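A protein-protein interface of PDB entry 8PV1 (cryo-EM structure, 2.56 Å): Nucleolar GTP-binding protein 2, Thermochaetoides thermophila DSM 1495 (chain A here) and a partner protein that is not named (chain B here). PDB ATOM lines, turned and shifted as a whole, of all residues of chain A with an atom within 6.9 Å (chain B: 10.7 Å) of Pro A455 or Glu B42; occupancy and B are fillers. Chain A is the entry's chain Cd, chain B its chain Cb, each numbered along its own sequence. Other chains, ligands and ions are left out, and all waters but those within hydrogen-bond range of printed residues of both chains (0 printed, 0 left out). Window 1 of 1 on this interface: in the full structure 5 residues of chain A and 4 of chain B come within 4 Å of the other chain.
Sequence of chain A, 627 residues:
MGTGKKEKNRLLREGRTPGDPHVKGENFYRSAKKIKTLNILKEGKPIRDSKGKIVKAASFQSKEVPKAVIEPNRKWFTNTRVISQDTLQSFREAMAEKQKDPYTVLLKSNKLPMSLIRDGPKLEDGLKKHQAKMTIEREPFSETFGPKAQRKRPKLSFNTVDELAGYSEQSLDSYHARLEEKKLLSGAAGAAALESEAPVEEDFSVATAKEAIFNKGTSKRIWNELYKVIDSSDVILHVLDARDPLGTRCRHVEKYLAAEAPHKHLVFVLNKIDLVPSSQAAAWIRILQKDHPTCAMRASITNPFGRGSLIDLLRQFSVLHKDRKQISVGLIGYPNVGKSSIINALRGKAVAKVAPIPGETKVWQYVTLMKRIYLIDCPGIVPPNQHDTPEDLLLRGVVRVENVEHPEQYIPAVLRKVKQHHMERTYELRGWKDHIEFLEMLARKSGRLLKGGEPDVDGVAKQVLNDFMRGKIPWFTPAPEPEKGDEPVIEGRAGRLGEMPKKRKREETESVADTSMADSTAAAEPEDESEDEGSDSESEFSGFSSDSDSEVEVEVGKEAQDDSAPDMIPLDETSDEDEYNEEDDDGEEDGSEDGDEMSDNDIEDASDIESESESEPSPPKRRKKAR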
ATOM      1  N   ILE A 436     -21.402 -14.240   7.523  1.00  0.00           N
ATOM      2  CA  ILE A 436     -20.228 -14.190   6.653  1.00  0.00           C
ATOM      3  C   ILE A 436     -19.094 -13.430   7.329  1.00  0.00           C
ATOM      4  O   ILE A 436     -17.942 -13.886   7.349  1.00  0.00           O
ATOM      5  CB  ILE A 436     -20.592 -13.569   5.292  1.00  0.00           C
ATOM      6  CG1 ILE A 436     -21.583 -14.463   4.551  1.00  0.00           C
ATOM      7  CG2 ILE A 436     -19.346 -13.347   4.451  1.00  0.00           C
ATOM      8  CD1 ILE A 436     -21.006 -15.806   4.161  1.00  0.00           C
ATOM      9  N   LEU A 439     -17.712 -15.565  10.211  1.00  0.00           N
ATOM     10  CA  LEU A 439     -16.803 -16.615   9.764  1.00  0.00           C
ATOM     11  C   LEU A 439     -15.468 -16.040   9.306  1.00  0.00           C
ATOM     12  O   LEU A 439     -14.415 -16.631   9.566  1.00  0.00           O
ATOM     13  CB  LEU A 439     -17.450 -17.438   8.649  1.00  0.00           C
ATOM     14  CG  LEU A 439     -18.695 -18.257   9.010  1.00  0.00           C
ATOM     15  CD1 LEU A 439     -19.292 -18.919   7.779  1.00  0.00           C
ATOM     16  CD2 LEU A 439     -18.407 -19.283  10.085  1.00  0.00           C
ATOM     17  N   GLU A 440     -15.487 -14.882   8.635  1.00  0.00           N
ATOM     18  CA  GLU A 440     -14.239 -14.253   8.206  1.00  0.00           C
ATOM     19  C   GLU A 440     -13.397 -13.800   9.395  1.00  0.00           C
ATOM     20  O   GLU A 440     -12.174 -13.995   9.410  1.00  0.00           O
ATOM     21  CB  GLU A 440     -14.534 -13.076   7.279  1.00  0.00           C
ATOM     22  CG  GLU A 440     -15.042 -13.482   5.908  1.00  0.00           C
ATOM     23  CD  GLU A 440     -15.541 -12.301   5.099  1.00  0.00           C
ATOM     24  OE1 GLU A 440     -15.500 -11.165   5.614  1.00  0.00           O
ATOM     25  OE2 GLU A 440     -15.976 -12.509   3.947  1.00  0.00           O
ATOM     26  N   MET A 441     -14.036 -13.198  10.405  1.00  0.00           N
ATOM     27  CA  MET A 441     -13.323 -12.784  11.610  1.00  0.00           C
ATOM     28  C   MET A 441     -12.746 -13.982  12.353  1.00  0.00           C
ATOM     29  O   MET A 441     -11.608 -13.935  12.833  1.00  0.00           O
ATOM     30  CB  MET A 441     -14.254 -11.984  12.525  1.00  0.00           C
ATOM     31  CG  MET A 441     -14.692 -10.635  11.978  1.00  0.00           C
ATOM     32  SD  MET A 441     -15.862  -9.784  13.057  1.00  0.00           S
ATOM     33  CE  MET A 441     -14.814  -9.338  14.433  1.00  0.00           C
ATOM     34  N   ALA A 443     -11.921 -16.870  11.007  1.00  0.00           N
ATOM     35  CA  ALA A 443     -10.833 -17.399  10.192  1.00  0.00           C
ATOM     36  C   ALA A 443      -9.559 -16.580  10.354  1.00  0.00           C
ATOM     37  O   ALA A 443      -8.464 -17.143  10.466  1.00  0.00           O
ATOM     38  CB  ALA A 443     -11.252 -17.443   8.724  1.00  0.00           C
ATOM     39  N   ARG A 444      -9.680 -15.250  10.375  1.00  0.00           N
ATOM     40  CA  ARG A 444      -8.495 -14.416  10.562  1.00  0.00           C
ATOM     41  C   ARG A 444      -7.942 -14.540  11.976  1.00  0.00           C
ATOM     42  O   ARG A 444      -6.726 -14.453  12.180  1.00  0.00           O
ATOM     43  CB  ARG A 444      -8.812 -12.959  10.236  1.00  0.00           C
ATOM     44  CG  ARG A 444      -9.250 -12.737   8.807  1.00  0.00           C
ATOM     45  CD  ARG A 444      -9.218 -11.270   8.438  1.00  0.00           C
ATOM     46  NE  ARG A 444      -9.984 -11.010   7.227  1.00  0.00           N
ATOM     47  CZ  ARG A 444     -11.215 -10.521   7.213  1.00  0.00           C
ATOM     48  NH1 ARG A 444     -11.846 -10.205   8.333  1.00  0.00           N
ATOM     49  NH2 ARG A 444     -11.830 -10.344   6.048  1.00  0.00           N
ATOM     50  N   ARG A 448      -7.109 -19.603   9.902  1.00  0.00           N
ATOM     51  CA  ARG A 448      -7.684 -20.451   8.858  1.00  0.00           C
ATOM     52  C   ARG A 448      -7.646 -19.680   7.543  1.00  0.00           C
ATOM     53  O   ARG A 448      -8.641 -19.120   7.074  1.00  0.00           O
ATOM     54  CB  ARG A 448      -9.101 -20.868   9.228  1.00  0.00           C
ATOM     55  CG  ARG A 448      -9.199 -21.824  10.408  1.00  0.00           C
ATOM     56  CD  ARG A 448      -8.531 -23.145  10.089  1.00  0.00           C
ATOM     57  NE  ARG A 448      -7.195 -23.234  10.662  1.00  0.00           N
ATOM     58  CZ  ARG A 448      -6.142 -23.712  10.017  1.00  0.00           C
ATOM     59  NH1 ARG A 448      -6.230 -24.125   8.765  1.00  0.00           N
ATOM     60  NH2 ARG A 448      -4.971 -23.766  10.639  1.00  0.00           N
ATOM     61  N   LEU A 449      -6.464 -19.655   6.934  1.00  0.00           N
ATOM     62  CA  LEU A 449      -6.215 -18.861   5.744  1.00  0.00           C
ATOM     63  C   LEU A 449      -5.834 -19.758   4.575  1.00  0.00           C
ATOM     64  O   LEU A 449      -5.195 -20.799   4.748  1.00  0.00           O
ATOM     65  CB  LEU A 449      -5.106 -17.833   5.990  1.00  0.00           C
ATOM     66  CG  LEU A 449      -5.271 -16.980   7.247  1.00  0.00           C
ATOM     67  CD1 LEU A 449      -4.002 -16.203   7.543  1.00  0.00           C
ATOM     68  CD2 LEU A 449      -6.459 -16.046   7.102  1.00  0.00           C
ATOM     69  N   LEU A 450      -6.239 -19.339   3.383  1.00  0.00           N
ATOM     70  CA  LEU A 450      -5.863 -20.008   2.148  1.00  0.00           C
ATOM     71  C   LEU A 450      -4.648 -19.299   1.553  1.00  0.00           C
ATOM     72  O   LEU A 450      -4.015 -18.462   2.202  1.00  0.00           O
ATOM     73  CB  LEU A 450      -7.050 -20.041   1.189  1.00  0.00           C
ATOM     74  CG  LEU A 450      -8.308 -20.736   1.713  1.00  0.00           C
ATOM     75  CD1 LEU A 450      -9.447 -20.630   0.716  1.00  0.00           C
ATOM     76  CD2 LEU A 450      -8.021 -22.189   2.045  1.00  0.00           C
ATOM     77  N   GLY A 452      -2.720 -16.575  -0.379  1.00  0.00           N
ATOM     78  CA  GLY A 452      -3.005 -15.164  -0.494  1.00  0.00           C
ATOM     79  C   GLY A 452      -3.782 -14.569   0.656  1.00  0.00           C
ATOM     80  O   GLY A 452      -4.457 -13.552   0.462  1.00  0.00           O
ATOM     81  N   GLY A 453      -3.738 -15.180   1.836  1.00  0.00           N
ATOM     82  CA  GLY A 453      -4.414 -14.640   2.997  1.00  0.00           C
ATOM     83  C   GLY A 453      -5.923 -14.687   2.953  1.00  0.00           C
ATOM     84  O   GLY A 453      -6.570 -14.025   3.772  1.00  0.00           O
ATOM     85  N   GLU A 454      -6.503 -15.438   2.027  1.00  0.00           N
ATOM     86  CA  GLU A 454      -7.954 -15.500   1.913  1.00  0.00           C
ATOM     87  C   GLU A 454      -8.528 -16.354   3.038  1.00  0.00           C
ATOM     88  O   GLU A 454      -8.033 -17.460   3.281  1.00  0.00           O
ATOM     89  CB  GLU A 454      -8.350 -16.066   0.553  1.00  0.00           C
ATOM     90  CG  GLU A 454      -9.844 -16.240   0.357  1.00  0.00           C
ATOM     91  CD  GLU A 454     -10.169 -17.160  -0.799  1.00  0.00           C
ATOM     92  OE1 GLU A 454      -9.225 -17.713  -1.403  1.00  0.00           O
ATOM     93  OE2 GLU A 454     -11.367 -17.332  -1.105  1.00  0.00           O
ATOM     94  N   PRO A 455      -9.543 -15.874   3.755  1.00  0.00           N
ATOM     95  CA  PRO A 455     -10.106 -16.654   4.864  1.00  0.00           C
ATOM     96  C   PRO A 455     -10.832 -17.903   4.376  1.00  0.00           C
ATOM     97  O   PRO A 455     -11.467 -17.901   3.320  1.00  0.00           O
ATOM     98  CB  PRO A 455     -11.067 -15.666   5.535  1.00  0.00           C
ATOM     99  CG  PRO A 455     -11.401 -14.684   4.471  1.00  0.00           C
ATOM    100  CD  PRO A 455     -10.168 -14.546   3.641  1.00  0.00           C
ATOM    101  N   ASP A 456     -10.730 -18.977   5.163  1.00  0.00           N
ATOM    102  CA  ASP A 456     -11.346 -20.263   4.828  1.00  0.00           C
ATOM    103  C   ASP A 456     -12.672 -20.382   5.574  1.00  0.00           C
ATOM    104  O   ASP A 456     -12.793 -21.046   6.611  1.00  0.00           O
ATOM    105  CB  ASP A 456     -10.404 -21.412   5.163  1.00  0.00           C
ATOM    106  CG  ASP A 456     -10.891 -22.745   4.624  1.00  0.00           C
ATOM    107  OD1 ASP A 456     -11.841 -22.760   3.815  1.00  0.00           O
ATOM    108  OD2 ASP A 456     -10.321 -23.784   5.016  1.00  0.00           O
ATOM    109  N   VAL A 457     -13.694 -19.732   5.011  1.00  0.00           N
ATOM    110  CA  VAL A 457     -15.015 -19.729   5.633  1.00  0.00           C
ATOM    111  C   VAL A 457     -15.642 -21.117   5.575  1.00  0.00           C
ATOM    112  O   VAL A 457     -16.433 -21.484   6.447  1.00  0.00           O
ATOM    113  CB  VAL A 457     -15.913 -18.656   4.987  1.00  0.00           C
ATOM    114  CG1 VAL A 457     -15.301 -17.280   5.177  1.00  0.00           C
ATOM    115  CG2 VAL A 457     -16.122 -18.930   3.507  1.00  0.00           C
ATOM    116  N   ASP A 458     -15.265 -21.920   4.574  1.00  0.00           N
ATOM    117  CA  ASP A 458     -15.721 -23.307   4.484  1.00  0.00           C
ATOM    118  C   ASP A 458     -15.264 -24.126   5.689  1.00  0.00           C
ATOM    119  O   ASP A 458     -16.082 -24.758   6.376  1.00  0.00           O
ATOM    120  CB  ASP A 458     -15.185 -23.919   3.190  1.00  0.00           C
ATOM    121  CG  ASP A 458     -15.680 -25.326   2.949  1.00  0.00           C
ATOM    122  OD1 ASP A 458     -16.822 -25.479   2.480  1.00  0.00           O
ATOM    123  OD2 ASP A 458     -14.926 -26.281   3.224  1.00  0.00           O
ATOM    124  N   VAL A 460     -14.011 -22.973   8.531  1.00  0.00           N
ATOM    125  CA  VAL A 460     -14.472 -22.368   9.777  1.00  0.00           C
ATOM    126  C   VAL A 460     -15.936 -22.719  10.033  1.00  0.00           C
ATOM    127  O   VAL A 460     -16.332 -22.988  11.174  1.00  0.00           O
ATOM    128  CB  VAL A 460     -14.219 -20.849   9.750  1.00  0.00           C
ATOM    129  CG1 VAL A 460     -14.927 -20.143  10.885  1.00  0.00           C
ATOM    130  CG2 VAL A 460     -12.742 -20.595   9.857  1.00  0.00           C
ATOM    131  N   LYS B  36      -9.526  -3.052 -10.189  1.00  0.00           N
ATOM    132  CA  LYS B  36      -9.862  -3.412  -8.816  1.00  0.00           C
ATOM    133  C   LYS B  36     -11.317  -3.846  -8.683  1.00  0.00           C
ATOM    134  O   LYS B  36     -11.642  -4.653  -7.806  1.00  0.00           O
ATOM    135  CB  LYS B  36      -9.561  -2.246  -7.879  1.00  0.00           C
ATOM    136  CG  LYS B  36      -8.079  -2.037  -7.632  1.00  0.00           C
ATOM    137  CD  LYS B  36      -7.834  -1.122  -6.450  1.00  0.00           C
ATOM    138  CE  LYS B  36      -6.364  -1.092  -6.084  1.00  0.00           C
ATOM    139  NZ  LYS B  36      -6.107  -0.258  -4.882  1.00  0.00           N
ATOM    140  N   GLU B  37     -12.203  -3.325  -9.535  1.00  0.00           N
ATOM    141  CA  GLU B  37     -13.593  -3.766  -9.520  1.00  0.00           C
ATOM    142  C   GLU B  37     -13.746  -5.145 -10.142  1.00  0.00           C
ATOM    143  O   GLU B  37     -14.739  -5.833  -9.883  1.00  0.00           O
ATOM    144  CB  GLU B  37     -14.481  -2.755 -10.243  1.00  0.00           C
ATOM    145  CG  GLU B  37     -14.862  -1.550  -9.402  1.00  0.00           C
ATOM    146  CD  GLU B  37     -15.436  -0.419 -10.231  1.00  0.00           C
ATOM    147  OE1 GLU B  37     -15.357  -0.492 -11.474  1.00  0.00           O
ATOM    148  OE2 GLU B  37     -15.966   0.544  -9.639  1.00  0.00           O
ATOM    149  N   THR B  38     -12.784  -5.567 -10.963  1.00  0.00           N
ATOM    150  CA  THR B  38     -12.771  -6.959 -11.413  1.00  0.00           C
ATOM    151  C   THR B  38     -12.356  -7.952 -10.320  1.00  0.00           C
ATOM    152  O   THR B  38     -12.328  -9.158 -10.589  1.00  0.00           O
ATOM    153  CB  THR B  38     -11.855  -7.138 -12.631  1.00  0.00           C
ATOM    154  OG1 THR B  38     -10.509  -6.786 -12.285  1.00  0.00           O
ATOM    155  CG2 THR B  38     -12.336  -6.314 -13.815  1.00  0.00           C
ATOM    156  N   LYS B  39     -12.033  -7.492  -9.112  1.00  0.00           N
ATOM    157  CA  LYS B  39     -11.677  -8.356  -7.995  1.00  0.00           C
ATOM    158  C   LYS B  39     -12.703  -8.226  -6.876  1.00  0.00           C
ATOM    159  O   LYS B  39     -13.614  -7.395  -6.928  1.00  0.00           O
ATOM    160  CB  LYS B  39     -10.283  -8.023  -7.445  1.00  0.00           C
ATOM    161  CG  LYS B  39      -9.139  -8.247  -8.418  1.00  0.00           C
ATOM    162  CD  LYS B  39      -8.951  -9.726  -8.707  1.00  0.00           C
ATOM    163  CE  LYS B  39      -7.705  -9.969  -9.535  1.00  0.00           C
ATOM    164  NZ  LYS B  39      -7.853  -9.435 -10.912  1.00  0.00           N
ATOM    165  N   ALA B  40     -12.541  -9.065  -5.856  1.00  0.00           N
ATOM    166  CA  ALA B  40     -13.377  -9.047  -4.661  1.00  0.00           C
ATOM    167  C   ALA B  40     -12.524  -8.604  -3.482  1.00  0.00           C
ATOM    168  O   ALA B  40     -11.457  -9.176  -3.238  1.00  0.00           O
ATOM    169  CB  ALA B  40     -13.991 -10.422  -4.399  1.00  0.00           C
ATOM    170  N   ALA B  41     -13.001  -7.594  -2.750  1.00  0.00           N
ATOM    171  CA  ALA B  41     -12.169  -6.944  -1.741  1.00  0.00           C
ATOM    172  C   ALA B  41     -11.933  -7.840  -0.530  1.00  0.00           C
ATOM    173  O   ALA B  41     -10.856  -7.799   0.078  1.00  0.00           O
ATOM    174  CB  ALA B  41     -12.805  -5.624  -1.311  1.00  0.00           C
ATOM    175  N   GLU B  42     -12.924  -8.652  -0.159  1.00  0.00           N
ATOM    176  CA  GLU B  42     -12.806  -9.449   1.057  1.00  0.00           C
ATOM    177  C   GLU B  42     -11.892 -10.656   0.891  1.00  0.00           C
ATOM    178  O   GLU B  42     -11.519 -11.276   1.893  1.00  0.00           O
ATOM    179  CB  GLU B  42     -14.189  -9.907   1.524  1.00  0.00           C
ATOM    180  CG  GLU B  42     -14.851 -10.929   0.615  1.00  0.00           C
ATOM    181  CD  GLU B  42     -15.770 -10.293  -0.409  1.00  0.00           C
ATOM    182  OE1 GLU B  42     -15.714  -9.057  -0.576  1.00  0.00           O
ATOM    183  OE2 GLU B  42     -16.551 -11.030  -1.046  1.00  0.00           O
ATOM    184  N   ASP B  43     -11.524 -11.009  -0.338  1.00  0.00           N
ATOM    185  CA  ASP B  43     -10.672 -12.162  -0.591  1.00  0.00           C
ATOM    186  C   ASP B  43      -9.220 -11.789  -0.864  1.00  0.00           C
ATOM    187  O   ASP B  43      -8.415 -12.675  -1.165  1.00  0.00           O
ATOM    188  CB  ASP B  43     -11.223 -12.973  -1.766  1.00  0.00           C
ATOM    189  CG  ASP B  43     -12.540 -13.647  -1.439  1.00  0.00           C
ATOM    190  OD1 ASP B  43     -12.966 -13.583  -0.268  1.00  0.00           O
ATOM    191  OD2 ASP B  43     -13.150 -14.241  -2.354  1.00  0.00           O
ATOM    192  N   LEU B  44      -8.868 -10.512  -0.770  1.00  0.00           N
ATOM    193  CA  LEU B  44      -7.540  -9.981  -1.029  1.00  0.00           C
ATOM    194  C   LEU B  44      -6.704  -9.970   0.246  1.00  0.00           C
ATOM    195  O   LEU B  44      -7.254  -9.980   1.352  1.00  0.00           O
ATOM    196  CB  LEU B  44      -7.641  -8.558  -1.590  1.00  0.00           C
ATOM    197  CG  LEU B  44      -8.262  -8.452  -2.981  1.00  0.00           C
ATOM    198  CD1 LEU B  44      -8.489  -7.003  -3.359  1.00  0.00           C
ATOM    199  CD2 LEU B  44      -7.395  -9.147  -4.012  1.00  0.00           C
ATOM    200  N   PRO B  45      -5.375  -9.991   0.127  1.00  0.00           N
ATOM    201  CA  PRO B  45      -4.527  -9.800   1.311  1.00  0.00           C
ATOM    202  C   PRO B  45      -4.746  -8.428   1.936  1.00  0.00           C
ATOM    203  O   PRO B  45      -4.742  -7.405   1.249  1.00  0.00           O
ATOM    204  CB  PRO B  45      -3.106  -9.941   0.756  1.00  0.00           C
ATOM    205  CG  PRO B  45      -3.250 -10.716  -0.493  1.00  0.00           C
ATOM    206  CD  PRO B  45      -4.596 -10.398  -1.055  1.00  0.00           C
ATOM    207  N   GLY B  46      -4.930  -8.417   3.254  1.00  0.00           N
ATOM    208  CA  GLY B  46      -5.178  -7.179   3.970  1.00  0.00           C
ATOM    209  C   GLY B  46      -6.462  -6.481   3.594  1.00  0.00           C
ATOM    210  O   GLY B  46      -6.551  -5.257   3.732  1.00  0.00           O
ATOM    211  N   LEU B  47      -7.455  -7.231   3.104  1.00  0.00           N
ATOM    212  CA  LEU B  47      -8.743  -6.727   2.624  1.00  0.00           C
ATOM    213  C   LEU B  47      -8.588  -5.721   1.485  1.00  0.00           C
ATOM    214  O   LEU B  47      -9.439  -4.845   1.308  1.00  0.00           O
ATOM    215  CB  LEU B  47      -9.584  -6.114   3.756  1.00  0.00           C
ATOM    216  CG  LEU B  47     -10.339  -7.015   4.744  1.00  0.00           C
ATOM    217  CD1 LEU B  47      -9.413  -7.736   5.717  1.00  0.00           C
ATOM    218  CD2 LEU B  47     -11.379  -6.204   5.503  1.00  0.00           C
ATOM    219  N   GLY B  48      -7.513  -5.832   0.705  1.00  0.00           N
ATOM    220  CA  GLY B  48      -7.264  -4.933  -0.401  1.00  0.00           C
ATOM    221  C   GLY B  48      -6.717  -3.575  -0.020  1.00  0.00           C
ATOM    222  O   GLY B  48      -6.567  -2.719  -0.901  1.00  0.00           O
ATOM    223  N   LEU B  49      -6.405  -3.348   1.255  1.00  0.00           N
ATOM    224  CA  LEU B  49      -6.006  -2.025   1.713  1.00  0.00           C
ATOM    225  C   LEU B  49      -4.557  -1.685   1.392  1.00  0.00           C
ATOM    226  O   LEU B  49      -4.201  -0.502   1.392  1.00  0.00           O
ATOM    227  CB  LEU B  49      -6.236  -1.908   3.220  1.00  0.00           C
ATOM    228  CG  LEU B  49      -7.702  -1.808   3.639  1.00  0.00           C
ATOM    229  CD1 LEU B  49      -7.817  -1.716   5.150  1.00  0.00           C
ATOM    230  CD2 LEU B  49      -8.371  -0.621   2.969  1.00  0.00           C
ATOM    231  N   TRP B  58      -1.084  -7.236  -4.176  1.00  0.00           N
ATOM    232  CA  TRP B  58      -1.665  -6.949  -2.874  1.00  0.00           C
ATOM    233  C   TRP B  58      -0.807  -7.556  -1.771  1.00  0.00           C
ATOM    234  O   TRP B  58      -0.141  -8.575  -1.968  1.00  0.00           O
ATOM    235  CB  TRP B  58      -3.094  -7.487  -2.778  1.00  0.00           C
ATOM    236  CG  TRP B  58      -4.113  -6.597  -3.415  1.00  0.00           C
ATOM    237  CD1 TRP B  58      -4.680  -5.483  -2.873  1.00  0.00           C
ATOM    238  CD2 TRP B  58      -4.689  -6.748  -4.717  1.00  0.00           C
ATOM    239  NE1 TRP B  58      -5.571  -4.928  -3.756  1.00  0.00           N
ATOM    240  CE2 TRP B  58      -5.597  -5.687  -4.895  1.00  0.00           C
ATOM    241  CE3 TRP B  58      -4.523  -7.675  -5.749  1.00  0.00           C
ATOM    242  CZ2 TRP B  58      -6.335  -5.526  -6.065  1.00  0.00           C
ATOM    243  CZ3 TRP B  58      -5.258  -7.515  -6.909  1.00  0.00           C
ATOM    244  CH2 TRP B  58      -6.152  -6.449  -7.057  1.00  0.00           C
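NH2 of Arg A444 lies within salt-bridge range of OE1 of Glu A440, at 3.8 Å.
Among the printed residues, merely in contact across the chains: Glu A440 with Glu B42 (3.9 Å), Arg A444 with Leu B47 (3.6 Å), Gly A452 with Pro B45 (3.2 Å), Glu A454 with Asp B43 (3.8 Å) and Pro A455 with Glu B42 (3.9 Å).
Glu A440 touches just one residue of chain B: Glu B42. No residue of chain B comes within 4 Å of Leu A450. Printed residues of chain B within 4 Å of Gly A452: Pro B45 (3.2 Å). No residue of chain B comes within 4 Å of Gly A453. Glu A454 touches just one residue of chain B: Asp B43 (3.8 Å). Printed residues of chain B within 4 Å of Pro A455: Glu B42. No residue of chain B comes within 4 Å of Asp A456. Of the printed residues of chain A, Glu B42 touches Glu A440 and Pro A455. Of the printed residues of chain A, Asp B43 touches Glu A454. Of the printed residues of chain A, Pro B45 touches Gly A452 (3.2 Å). Of the printed residues of chain A, Leu B47 touches Arg A444. The nearest residue of chain B that does not touch Pro A455 is Asp B43 (4.9 Å). The nearest residue of chain A that does not touch Glu B42 is Arg A444 (4.3 Å). The nearest printed residue of chain B that does not touch Gly A452 is Leu B44 (4.2 Å).
Of the 17 printed residues of chain A, 5 touch a printed residue of chain B. Hydrophobic or aromatic side chains of chain A that line the printed part of chain B: Pro A455. Among the printed residues, no Asp or Glu carboxylate lies within 4 Å of a Lys or Arg side-chain nitrogen of the other chain.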
